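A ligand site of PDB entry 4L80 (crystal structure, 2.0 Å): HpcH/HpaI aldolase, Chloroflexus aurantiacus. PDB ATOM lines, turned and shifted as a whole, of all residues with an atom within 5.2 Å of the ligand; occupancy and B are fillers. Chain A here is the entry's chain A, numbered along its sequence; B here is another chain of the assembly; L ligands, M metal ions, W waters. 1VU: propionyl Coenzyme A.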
ATOM      1  N   HIS A  32      19.837  16.101   7.192  1.00  0.00           N
ATOM      2  CA  HIS A  32      20.050  16.130   8.639  1.00  0.00           C
ATOM      3  C   HIS A  32      19.219  17.185   9.343  1.00  0.00           C
ATOM      4  O   HIS A  32      19.397  18.390   9.118  1.00  0.00           O
ATOM      5  CB  HIS A  32      21.532  16.304   8.990  1.00  0.00           C
ATOM      6  CG  HIS A  32      21.791  16.222  10.463  1.00  0.00           C
ATOM      7  ND1 HIS A  32      21.698  15.040  11.161  1.00  0.00           N
ATOM      8  CD2 HIS A  32      22.121  17.176  11.371  1.00  0.00           C
ATOM      9  CE1 HIS A  32      21.960  15.270  12.437  1.00  0.00           C
ATOM     10  NE2 HIS A  32      22.227  16.553  12.587  1.00  0.00           N
ATOM     11  N   PHE A  33      18.316  16.729  10.203  1.00  0.00           N
ATOM     12  CA  PHE A  33      17.446  17.611  10.968  1.00  0.00           C
ATOM     13  C   PHE A  33      18.115  18.046  12.273  1.00  0.00           C
ATOM     14  O   PHE A  33      18.788  17.243  12.929  1.00  0.00           O
ATOM     15  CB  PHE A  33      16.124  16.899  11.296  1.00  0.00           C
ATOM     16  CG  PHE A  33      15.035  17.170  10.297  1.00  0.00           C
ATOM     17  CD1 PHE A  33      15.166  16.763   8.980  1.00  0.00           C
ATOM     18  CD2 PHE A  33      13.876  17.814  10.686  1.00  0.00           C
ATOM     19  CE1 PHE A  33      14.165  17.012   8.067  1.00  0.00           C
ATOM     20  CE2 PHE A  33      12.862  18.057   9.774  1.00  0.00           C
ATOM     21  CZ  PHE A  33      13.015  17.656   8.461  1.00  0.00           C
ATOM     22  N   PHE A  34      17.910  19.293  12.650  1.00  0.00           N
ATOM     23  CA  PHE A  34      18.409  19.786  13.935  1.00  0.00           C
ATOM     24  C   PHE A  34      17.463  20.816  14.533  1.00  0.00           C
ATOM     25  O   PHE A  34      16.833  21.579  13.798  1.00  0.00           O
ATOM     26  CB  PHE A  34      19.826  20.348  13.801  1.00  0.00           C
ATOM     27  CG  PHE A  34      19.894  21.710  13.152  1.00  0.00           C
ATOM     28  CD1 PHE A  34      19.962  22.864  13.922  1.00  0.00           C
ATOM     29  CD2 PHE A  34      19.902  21.839  11.767  1.00  0.00           C
ATOM     30  CE1 PHE A  34      20.029  24.105  13.337  1.00  0.00           C
ATOM     31  CE2 PHE A  34      19.973  23.088  11.175  1.00  0.00           C
ATOM     32  CZ  PHE A  34      20.033  24.228  11.957  1.00  0.00           C
ATOM     33  N   PRO A  35      17.345  20.831  15.871  1.00  0.00           N
ATOM     34  CA  PRO A  35      16.567  21.840  16.576  1.00  0.00           C
ATOM     35  C   PRO A  35      17.411  23.093  16.809  1.00  0.00           C
ATOM     36  O   PRO A  35      18.344  23.070  17.613  1.00  0.00           O
ATOM     37  CB  PRO A  35      16.224  21.158  17.896  1.00  0.00           C
ATOM     38  CG  PRO A  35      17.337  20.208  18.135  1.00  0.00           C
ATOM     39  CD  PRO A  35      17.850  19.781  16.778  1.00  0.00           C
ATOM     40  N   LYS A  40      23.820  24.373  22.289  1.00  0.00           N
ATOM     41  CA  LYS A  40      24.828  23.325  22.218  1.00  0.00           C
ATOM     42  C   LYS A  40      24.912  22.717  20.811  1.00  0.00           C
ATOM     43  O   LYS A  40      26.003  22.512  20.285  1.00  0.00           O
ATOM     44  CB  LYS A  40      24.511  22.228  23.232  1.00  0.00           C
ATOM     45  CG  LYS A  40      25.261  20.933  23.010  1.00  0.00           C
ATOM     46  CD  LYS A  40      24.745  19.846  23.949  1.00  0.00           C
ATOM     47  CE  LYS A  40      25.433  18.520  23.668  1.00  0.00           C
ATOM     48  NZ  LYS A  40      24.934  17.439  24.559  1.00  0.00           N
ATOM     49  N   ILE A  41      23.758  22.448  20.222  1.00  0.00           N
ATOM     50  CA  ILE A  41      23.686  21.882  18.870  1.00  0.00           C
ATOM     51  C   ILE A  41      24.049  22.925  17.828  1.00  0.00           C
ATOM     52  O   ILE A  41      24.762  22.646  16.866  1.00  0.00           O
ATOM     53  CB  ILE A  41      22.295  21.288  18.578  1.00  0.00           C
ATOM     54  CG1 ILE A  41      22.018  20.109  19.513  1.00  0.00           C
ATOM     55  CG2 ILE A  41      22.176  20.839  17.126  1.00  0.00           C
ATOM     56  CD1 ILE A  41      20.695  19.409  19.267  1.00  0.00           C
ATOM     57  N   ARG A  44      27.640  23.399  17.201  1.00  0.00           N
ATOM     58  CA  ARG A  44      28.286  22.289  16.507  1.00  0.00           C
ATOM     59  C   ARG A  44      27.873  22.200  15.036  1.00  0.00           C
ATOM     60  O   ARG A  44      28.496  21.475  14.259  1.00  0.00           O
ATOM     61  CB  ARG A  44      27.968  20.971  17.213  1.00  0.00           C
ATOM     62  CG  ARG A  44      28.533  20.876  18.618  1.00  0.00           C
ATOM     63  CD  ARG A  44      29.514  19.717  18.735  1.00  0.00           C
ATOM     64  NE  ARG A  44      30.658  19.882  17.835  1.00  0.00           N
ATOM     65  CZ  ARG A  44      31.469  18.900  17.475  1.00  0.00           C
ATOM     66  NH1 ARG A  44      31.268  17.670  17.933  1.00  0.00           N
ATOM     67  NH2 ARG A  44      32.479  19.134  16.656  1.00  0.00           N
ATOM     68  N   ILE A  45      26.831  22.937  14.662  1.00  0.00           N
ATOM     69  CA  ILE A  45      26.291  22.903  13.295  1.00  0.00           C
ATOM     70  C   ILE A  45      27.316  23.063  12.162  1.00  0.00           C
ATOM     71  O   ILE A  45      27.314  22.258  11.231  1.00  0.00           O
ATOM     72  CB  ILE A  45      25.109  23.894  13.120  1.00  0.00           C
ATOM     73  CG1 ILE A  45      23.840  23.328  13.756  1.00  0.00           C
ATOM     74  CG2 ILE A  45      24.865  24.181  11.653  1.00  0.00           C
ATOM     75  CD1 ILE A  45      23.391  22.024  13.118  1.00  0.00           C
ATOM     76  N   VAL A  48      29.026  19.787  11.811  1.00  0.00           N
ATOM     77  CA  VAL A  48      28.104  18.767  11.308  1.00  0.00           C
ATOM     78  C   VAL A  48      27.824  18.943   9.827  1.00  0.00           C
ATOM     79  O   VAL A  48      27.790  17.971   9.066  1.00  0.00           O
ATOM     80  CB  VAL A  48      26.785  18.787  12.097  1.00  0.00           C
ATOM     81  CG1 VAL A  48      25.746  17.876  11.454  1.00  0.00           C
ATOM     82  CG2 VAL A  48      27.018  18.388  13.547  1.00  0.00           C
ATOM     83  N   ASN A  58      14.716  22.648  11.816  1.00  0.00           N
ATOM     84  CA  ASN A  58      13.349  22.245  12.126  1.00  0.00           C
ATOM     85  C   ASN A  58      12.639  23.234  13.051  1.00  0.00           C
ATOM     86  O   ASN A  58      13.120  23.529  14.140  1.00  0.00           O
ATOM     87  CB  ASN A  58      13.332  20.858  12.765  1.00  0.00           C
ATOM     88  CG  ASN A  58      11.944  20.422  13.187  1.00  0.00           C
ATOM     89  OD1 ASN A  58      10.971  20.626  12.456  1.00  0.00           O
ATOM     90  ND2 ASN A  58      11.839  19.824  14.370  1.00  0.00           N
ATOM     91  N   ASP A  61       7.173  20.203  14.319  1.00  0.00           N
ATOM     92  CA  ASP A  61       7.077  19.172  15.343  1.00  0.00           C
ATOM     93  C   ASP A  61       8.435  18.840  15.953  1.00  0.00           C
ATOM     94  O   ASP A  61       9.450  18.868  15.255  1.00  0.00           O
ATOM     95  CB  ASP A  61       6.416  17.901  14.776  1.00  0.00           C
ATOM     96  CG  ASP A  61       4.956  18.115  14.425  1.00  0.00           C
ATOM     97  OD1 ASP A  61       4.423  19.207  14.702  1.00  0.00           O
ATOM     98  OD2 ASP A  61       4.346  17.173  13.877  1.00  0.00           O
ATOM     99  N   ALA A  62       8.403  18.528  17.252  1.00  0.00           N
ATOM    100  CA  ALA A  62       9.570  18.335  18.128  1.00  0.00           C
ATOM    101  C   ALA A  62      10.112  19.645  18.706  1.00  0.00           C
ATOM    102  O   ALA A  62      10.936  19.624  19.619  1.00  0.00           O
ATOM    103  CB  ALA A  62      10.693  17.516  17.457  1.00  0.00           C
ATOM    104  N   ARG A  92      12.333  23.286   7.682  1.00  0.00           N
ATOM    105  CA  ARG A  92      10.941  22.906   7.821  1.00  0.00           C
ATOM    106  C   ARG A  92      10.241  23.930   8.693  1.00  0.00           C
ATOM    107  O   ARG A  92      10.504  24.024   9.887  1.00  0.00           O
ATOM    108  CB  ARG A  92      10.800  21.508   8.430  1.00  0.00           C
ATOM    109  CG  ARG A  92       9.342  21.063   8.533  1.00  0.00           C
ATOM    110  CD  ARG A  92       9.202  19.607   8.933  1.00  0.00           C
ATOM    111  NE  ARG A  92       9.408  19.395  10.357  1.00  0.00           N
ATOM    112  CZ  ARG A  92       9.113  18.266  10.993  1.00  0.00           C
ATOM    113  NH1 ARG A  92       8.585  17.246  10.333  1.00  0.00           N
ATOM    114  NH2 ARG A  92       9.350  18.150  12.298  1.00  0.00           N
ATOM    115  N   ALA A 183       5.099   9.067  10.790  1.00  0.00           N
ATOM    116  CA  ALA A 183       4.438   9.293  12.072  1.00  0.00           C
ATOM    117  C   ALA A 183       3.080   9.974  11.893  1.00  0.00           C
ATOM    118  O   ALA A 183       2.059   9.434  12.288  1.00  0.00           O
ATOM    119  CB  ALA A 183       5.329  10.090  13.011  1.00  0.00           C
ATOM    120  N   VAL A 196       7.629   4.808  14.292  1.00  0.00           N
ATOM    121  CA  VAL A 196       7.932   5.757  13.220  1.00  0.00           C
ATOM    122  C   VAL A 196       8.781   5.067  12.163  1.00  0.00           C
ATOM    123  O   VAL A 196      10.006   5.058  12.252  1.00  0.00           O
ATOM    124  CB  VAL A 196       8.659   7.000  13.770  1.00  0.00           C
ATOM    125  CG1 VAL A 196       8.909   8.004  12.657  1.00  0.00           C
ATOM    126  CG2 VAL A 196       7.851   7.629  14.887  1.00  0.00           C
ATOM    127  N   PRO A 246      11.814  10.365   8.557  1.00  0.00           N
ATOM    128  CA  PRO A 246      12.494   9.976   9.800  1.00  0.00           C
ATOM    129  C   PRO A 246      12.337   8.493  10.126  1.00  0.00           C
ATOM    130  O   PRO A 246      11.306   7.880   9.831  1.00  0.00           O
ATOM    131  CB  PRO A 246      11.751  10.791  10.854  1.00  0.00           C
ATOM    132  CG  PRO A 246      10.354  10.884  10.317  1.00  0.00           C
ATOM    133  CD  PRO A 246      10.499  10.966   8.809  1.00  0.00           C
ATOM    134  N   ILE A 250      16.085   5.677  17.045  1.00  0.00           N
ATOM    135  CA  ILE A 250      17.459   6.122  16.868  1.00  0.00           C
ATOM    136  C   ILE A 250      18.489   5.060  17.253  1.00  0.00           C
ATOM    137  O   ILE A 250      19.543   4.950  16.627  1.00  0.00           O
ATOM    138  CB  ILE A 250      17.732   7.400  17.684  1.00  0.00           C
ATOM    139  CG1 ILE A 250      16.639   8.440  17.443  1.00  0.00           C
ATOM    140  CG2 ILE A 250      19.098   7.980  17.340  1.00  0.00           C
ATOM    141  CD1 ILE A 250      16.554   8.912  16.010  1.00  0.00           C
ATOM    142  N   LYS A 251      18.172   4.282  18.275  1.00  0.00           N
ATOM    143  CA  LYS A 251      19.098   3.286  18.809  1.00  0.00           C
ATOM    144  C   LYS A 251      19.176   2.019  17.950  1.00  0.00           C
ATOM    145  O   LYS A 251      20.205   1.339  17.937  1.00  0.00           O
ATOM    146  CB  LYS A 251      18.733   2.925  20.254  1.00  0.00           C
ATOM    147  CG  LYS A 251      18.828   4.077  21.236  1.00  0.00           C
ATOM    148  CD  LYS A 251      20.251   4.590  21.362  1.00  0.00           C
ATOM    149  CE  LYS A 251      20.369   5.663  22.452  1.00  0.00           C
ATOM    150  NZ  LYS A 251      19.528   6.858  22.160  1.00  0.00           N
ATOM    151  N   TRP A 272      16.070  11.136   6.081  1.00  0.00           N
ATOM    152  CA  TRP A 272      16.420  12.074   7.133  1.00  0.00           C
ATOM    153  C   TRP A 272      17.341  11.392   8.138  1.00  0.00           C
ATOM    154  O   TRP A 272      17.267  10.178   8.342  1.00  0.00           O
ATOM    155  CB  TRP A 272      15.183  12.548   7.887  1.00  0.00           C
ATOM    156  CG  TRP A 272      14.151  13.248   7.054  1.00  0.00           C
ATOM    157  CD1 TRP A 272      14.162  13.448   5.715  1.00  0.00           C
ATOM    158  CD2 TRP A 272      12.939  13.840   7.546  1.00  0.00           C
ATOM    159  NE1 TRP A 272      13.032  14.137   5.325  1.00  0.00           N
ATOM    160  CE2 TRP A 272      12.268  14.386   6.431  1.00  0.00           C
ATOM    161  CE3 TRP A 272      12.371  13.966   8.814  1.00  0.00           C
ATOM    162  CZ2 TRP A 272      11.042  15.042   6.560  1.00  0.00           C
ATOM    163  CZ3 TRP A 272      11.152  14.621   8.930  1.00  0.00           C
ATOM    164  CH2 TRP A 272      10.507  15.143   7.807  1.00  0.00           C
ATOM    165  N   LEU A 274      18.072  12.044  12.250  1.00  0.00           N
ATOM    166  CA  LEU A 274      17.544  12.797  13.384  1.00  0.00           C
ATOM    167  C   LEU A 274      18.606  12.984  14.456  1.00  0.00           C
ATOM    168  O   LEU A 274      18.412  13.728  15.415  1.00  0.00           O
ATOM    169  CB  LEU A 274      16.331  12.084  13.980  1.00  0.00           C
ATOM    170  CG  LEU A 274      15.187  11.756  13.007  1.00  0.00           C
ATOM    171  CD1 LEU A 274      14.069  11.034  13.740  1.00  0.00           C
ATOM    172  CD2 LEU A 274      14.665  13.021  12.340  1.00  0.00           C
ATOM    173  N   ALA A 275      19.731  12.287  14.295  1.00  0.00           N
ATOM    174  CA  ALA A 275      20.837  12.319  15.230  1.00  0.00           C
ATOM    175  C   ALA A 275      22.112  11.962  14.467  1.00  0.00           C
ATOM    176  O   ALA A 275      22.021  11.342  13.417  1.00  0.00           O
ATOM    177  CB  ALA A 275      20.595  11.337  16.371  1.00  0.00           C
ATOM    178  N   PRO A 276      23.287  12.356  14.979  1.00  0.00           N
ATOM    179  CA  PRO A 276      24.535  12.130  14.242  1.00  0.00           C
ATOM    180  C   PRO A 276      24.804  10.663  13.882  1.00  0.00           C
ATOM    181  O   PRO A 276      25.393  10.416  12.837  1.00  0.00           O
ATOM    182  CB  PRO A 276      25.600  12.642  15.217  1.00  0.00           C
ATOM    183  CG  PRO A 276      24.903  13.679  16.008  1.00  0.00           C
ATOM    184  CD  PRO A 276      23.512  13.157  16.203  1.00  0.00           C
ATOM    185  N   ASN A 277      24.383   9.724  14.720  1.00  0.00           N
ATOM    186  CA  ASN A 277      24.611   8.311  14.439  1.00  0.00           C
ATOM    187  C   ASN A 277      23.904   7.844  13.154  1.00  0.00           C
ATOM    188  O   ASN A 277      24.343   6.888  12.520  1.00  0.00           O
ATOM    189  CB  ASN A 277      24.196   7.436  15.613  1.00  0.00           C
ATOM    190  CG  ASN A 277      22.692   7.393  15.815  1.00  0.00           C
ATOM    191  OD1 ASN A 277      22.035   8.417  15.820  1.00  0.00           O
ATOM    192  ND2 ASN A 277      22.155   6.192  15.979  1.00  0.00           N
ATOM    193  N   VAL B 309       9.532  17.464  22.156  1.00  0.00           N
ATOM    194  CA  VAL B 309      10.290  16.253  21.852  1.00  0.00           C
ATOM    195  C   VAL B 309      10.539  15.455  23.136  1.00  0.00           C
ATOM    196  O   VAL B 309      10.562  16.010  24.232  1.00  0.00           O
ATOM    197  CB  VAL B 309      11.624  16.587  21.150  1.00  0.00           C
ATOM    198  CG1 VAL B 309      12.617  17.204  22.126  1.00  0.00           C
ATOM    199  CG2 VAL B 309      12.223  15.346  20.477  1.00  0.00           C
ATOM    200  N   MET B 311      12.317  11.283  24.560  1.00  0.00           N
ATOM    201  CA  MET B 311      12.853   9.950  24.281  1.00  0.00           C
ATOM    202  C   MET B 311      12.265   8.941  25.256  1.00  0.00           C
ATOM    203  O   MET B 311      12.228   9.175  26.466  1.00  0.00           O
ATOM    204  CB  MET B 311      14.388   9.935  24.395  1.00  0.00           C
ATOM    205  CG  MET B 311      15.116  10.825  23.401  1.00  0.00           C
ATOM    206  SD  MET B 311      15.005  10.275  21.682  1.00  0.00           S
ATOM    207  CE  MET B 311      15.703   8.630  21.792  1.00  0.00           C
ATOM    208  N   MET B 316      12.556   8.151  19.813  1.00  0.00           N
ATOM    209  CA  MET B 316      12.186   9.554  19.759  1.00  0.00           C
ATOM    210  C   MET B 316      10.677   9.765  19.650  1.00  0.00           C
ATOM    211  O   MET B 316      10.026   9.174  18.789  1.00  0.00           O
ATOM    212  CB  MET B 316      12.900  10.260  18.604  1.00  0.00           C
ATOM    213  CG  MET B 316      12.094  11.395  18.025  1.00  0.00           C
ATOM    214  SD  MET B 316      13.045  12.656  17.182  1.00  0.00           S
ATOM    215  CE  MET B 316      11.800  13.938  17.118  1.00  0.00           C
ATOM    216  N   ASP B 318       7.490  12.831  19.597  1.00  0.00           N
ATOM    217  CA  ASP B 318       7.188  14.242  19.369  1.00  0.00           C
ATOM    218  C   ASP B 318       5.702  14.487  19.165  1.00  0.00           C
ATOM    219  O   ASP B 318       4.870  13.674  19.553  1.00  0.00           O
ATOM    220  CB  ASP B 318       7.997  14.805  18.187  1.00  0.00           C
ATOM    221  CG  ASP B 318       7.814  14.007  16.913  1.00  0.00           C
ATOM    222  OD1 ASP B 318       8.801  13.882  16.159  1.00  0.00           O
ATOM    223  OD2 ASP B 318       6.695  13.517  16.627  1.00  0.00           O
ATOM    224  N   ALA B 320       3.907  14.332  16.569  1.00  0.00           N
ATOM    225  CA  ALA B 320       3.281  13.348  15.687  1.00  0.00           C
ATOM    226  C   ALA B 320       3.005  12.019  16.378  1.00  0.00           C
ATOM    227  O   ALA B 320       1.929  11.447  16.227  1.00  0.00           O
ATOM    228  CB  ALA B 320       4.115  13.156  14.430  1.00  0.00           C
ATOM    229  N   THR B 321       3.983  11.523  17.135  1.00  0.00           N
ATOM    230  CA  THR B 321       3.771  10.288  17.890  1.00  0.00           C
ATOM    231  C   THR B 321       2.718  10.513  18.970  1.00  0.00           C
ATOM    232  O   THR B 321       2.020   9.582  19.369  1.00  0.00           O
ATOM    233  CB  THR B 321       5.086   9.733  18.520  1.00  0.00           C
ATOM    234  OG1 THR B 321       5.543  10.605  19.556  1.00  0.00           O
ATOM    235  CG2 THR B 321       6.168   9.584  17.462  1.00  0.00           C
HETATM  236  O14 1VU L   1      27.661  16.561  23.382  1.00  0.00           O
HETATM  237  P2  1VU L   1      27.959  16.302  21.998  1.00  0.00           P
HETATM  238  O15 1VU L   1      28.837  15.024  21.816  1.00  0.00           O
HETATM  239  O16 1VU L   1      28.683  17.563  21.325  1.00  0.00           O
HETATM  240  O13 1VU L   1      26.518  16.229  21.313  1.00  0.00           O
HETATM  241  C23 1VU L   1      25.552  15.215  21.324  1.00  0.00           C
HETATM  242  C22 1VU L   1      24.226  15.835  20.922  1.00  0.00           C
HETATM  243  O12 1VU L   1      24.031  17.125  21.467  1.00  0.00           O
HETATM  244  C16 1VU L   1      24.394  15.972  19.424  1.00  0.00           C
HETATM  245  N2  1VU L   1      23.144  15.924  18.653  1.00  0.00           N
HETATM  246  C21 1VU L   1      22.991  16.509  17.493  1.00  0.00           C
HETATM  247  N6  1VU L   1      23.803  17.243  16.729  1.00  0.00           N
HETATM  248  C20 1VU L   1      23.390  17.730  15.562  1.00  0.00           C
HETATM  249  N5  1VU L   1      22.156  17.512  15.137  1.00  0.00           N
HETATM  250  C19 1VU L   1      21.303  16.767  15.829  1.00  0.00           C
HETATM  251  N4  1VU L   1      20.076  16.526  15.368  1.00  0.00           N
HETATM  252  C18 1VU L   1      21.719  16.251  17.047  1.00  0.00           C
HETATM  253  N3  1VU L   1      21.150  15.510  17.969  1.00  0.00           N
HETATM  254  C17 1VU L   1      22.027  15.307  18.964  1.00  0.00           C
HETATM  255  O11 1VU L   1      25.215  14.911  19.034  1.00  0.00           O
HETATM  256  C15 1VU L   1      25.833  14.313  20.154  1.00  0.00           C
HETATM  257  C14 1VU L   1      25.202  12.964  20.337  1.00  0.00           C
HETATM  258  O10 1VU L   1      23.902  13.081  20.869  1.00  0.00           O
HETATM  259  P1  1VU L   1      22.918  11.870  20.962  1.00  0.00           P
HETATM  260  O8  1VU L   1      23.138  11.023  19.843  1.00  0.00           O
HETATM  261  O9  1VU L   1      22.974  11.088  22.298  1.00  0.00           O
HETATM  262  O7  1VU L   1      21.467  12.432  20.884  1.00  0.00           O
HETATM  263  P   1VU L   1      20.694  12.895  22.136  1.00  0.00           P
HETATM  264  O5  1VU L   1      20.170  11.758  22.803  1.00  0.00           O
HETATM  265  O6  1VU L   1      21.540  13.895  23.023  1.00  0.00           O
HETATM  266  O4  1VU L   1      19.435  13.651  21.520  1.00  0.00           O
HETATM  267  C13 1VU L   1      18.465  12.911  20.785  1.00  0.00           C
HETATM  268  C10 1VU L   1      17.444  13.816  20.103  1.00  0.00           C
HETATM  269  C11 1VU L   1      16.499  13.031  19.238  1.00  0.00           C
HETATM  270  C12 1VU L   1      16.685  14.490  21.222  1.00  0.00           C
HETATM  271  C9  1VU L   1      18.119  14.810  19.155  1.00  0.00           C
HETATM  272  O3  1VU L   1      18.967  14.065  18.329  1.00  0.00           O
HETATM  273  C8  1VU L   1      17.120  15.635  18.383  1.00  0.00           C
HETATM  274  O2  1VU L   1      16.449  16.427  18.973  1.00  0.00           O
HETATM  275  N1  1VU L   1      17.046  15.438  17.091  1.00  0.00           N
HETATM  276  C7  1VU L   1      16.224  16.140  16.158  1.00  0.00           C
HETATM  277  C6  1VU L   1      14.833  15.546  16.063  1.00  0.00           C
HETATM  278  C5  1VU L   1      13.998  16.163  14.981  1.00  0.00           C
HETATM  279  O1  1VU L   1      14.410  16.997  14.281  1.00  0.00           O
HETATM  280  N   1VU L   1      12.808  15.665  14.915  1.00  0.00           N
HETATM  281  C4  1VU L   1      11.805  16.142  14.020  1.00  0.00           C
HETATM  282  C3  1VU L   1      11.672  15.276  12.788  1.00  0.00           C
HETATM  283  S   1VU L   1      10.803  13.821  13.183  1.00  0.00           S
HETATM  284  C2  1VU L   1       9.179  14.193  13.235  1.00  0.00           C
HETATM  285  O   1VU L   1       8.780  15.322  13.171  1.00  0.00           O
HETATM  286  C1  1VU L   1       8.138  13.093  13.362  1.00  0.00           C
HETATM  287  C   1VU L   1       8.705  11.824  13.892  1.00  0.00           C
HETATM  288 MG    MG M   1       5.123  15.092  10.809  1.00  0.00          MG
HETATM  289  O   HOH W   1      14.304  19.177  15.680  1.00  0.00           O
HETATM  290  O   HOH W   2      14.188  18.152  18.230  1.00  0.00           O
HETATM  291  O   HOH W   3       5.750  15.313  12.928  1.00  0.00           O
HETATM  292  O   HOH W   4      26.257  18.192  17.641  1.00  0.00           O
HETATM  293  O   HOH W   5      25.962  19.144  20.372  1.00  0.00           O
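Water W1 lies within hydrogen-bond range of O1 of the ligand (2.6 Å) and ND2 of Asn 58 (2.9 Å). Water W5 lies within hydrogen-bond range of O12 of the ligand (3.0 Å) and O of Lys 40 (3.4 Å). Water W3 lies within hydrogen-bond range of the side-chain carboxylate of Asp 61 (2.5 Å) and an oxygen (O) of the ligand (3.0 Å).
O of the ligand lies close to OD1 of Asp 318 of chain B. CB of Phe 34 touches N5 of the ligand, 3.9 Å away. Pro 35 touches the ligand. Ile 41 touches the ligand. Arg 44 touches the ligand (CD to O16, 3.5 Å). Asn 58 touches the ligand (ND2 to C4, 3.7 Å). Asp 61 touches the ligand. CB of Ala 62 touches N of the ligand, at 3.8 Å. Ala 183 touches the ligand. CB of Pro 246 touches S of the ligand, 3.9 Å away. Trp 272 touches the ligand (CZ3 to C3, 3.9 Å). Ala 275 touches the ligand. CG of Pro 276 touches O11 of the ligand, at 3.3 Å. Met 311 of chain B touches the ligand (SD to C11, 3.98 Å). Hydrophobic or aromatic side chains within 4 Å of the ligand: His 32, Phe 33, Phe 34, Pro 35, Ile 41, Ala 62, Ala 183, Pro 246, Trp 272, Leu 274, Ala 275, Pro 276, Met 311 of chain B and Met 316 of chain B. Within 4 Å of the ligand: His 32, Phe 33, Phe 34, Pro 35, Lys 40, Ile 41, Arg 44, Asn 58, Asp 61, Ala 62, Arg 92, Ala 183, Pro 246, Trp 272, Leu 274, Ala 275, Pro 276, Met 311 of chain B, Met 316 of chain B and Asp 318 of chain B. The nearest printed residue that does not touch the ligand is Val 196 (4.02 Å).
The backbone NH (N) of Asp 318 of chain B is in hydrogen-bond range of the side-chain hydroxyl (OG1) of Thr 321 of chain B, 3.0 Å away. The backbone NH of Asn 58 is in hydrogen-bond range of the backbone carbonyl oxygen of Phe 34. The guanidinium group (NH2) of Arg 92 sits at hydrogen-bond distance from the backbone carbonyl oxygen (O) of Asp 61, 3.0 Å away. The guanidinium group (NE) of Arg 92 lies within hydrogen-bond range of the side-chain amide oxygen (OD1) of Asn 58 (2.9 Å). The backbone NH (N) of Met 316 of chain B sits close to the side-chain sulfur (SD) of Met 311 of chain B, at 3.7 Å. OD2 of Asp 318 of chain B sits at hydrogen-bond distance from N of Ala 320 of chain B (2.9 Å). The side-chain amide nitrogen (ND2) of Asn 58 lies within hydrogen-bond range of the backbone carbonyl oxygen (O) of Asp 61 (2.7 Å).
O of Phe 33 sits at hydrogen-bond distance from N4 of the ligand, 2.8 Å away. An oxygen (O14) of the ligand is in salt-bridge range of the side-chain amino group (NZ) of Lys 40 (3.1 Å). The side-chain sulfur (SD) of Met 316 of chain B lies close to a nitrogen (N) of the ligand (3.8 Å). A nitrogen (N1) of the ligand lies within hydrogen-bond range of the backbone carbonyl oxygen (O) of Leu 274, 2.8 Å away. NE2 of His 32 sits at hydrogen-bond distance from N5 of the ligand. O of the ligand is in hydrogen-bond range of NH2 of Arg 92.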
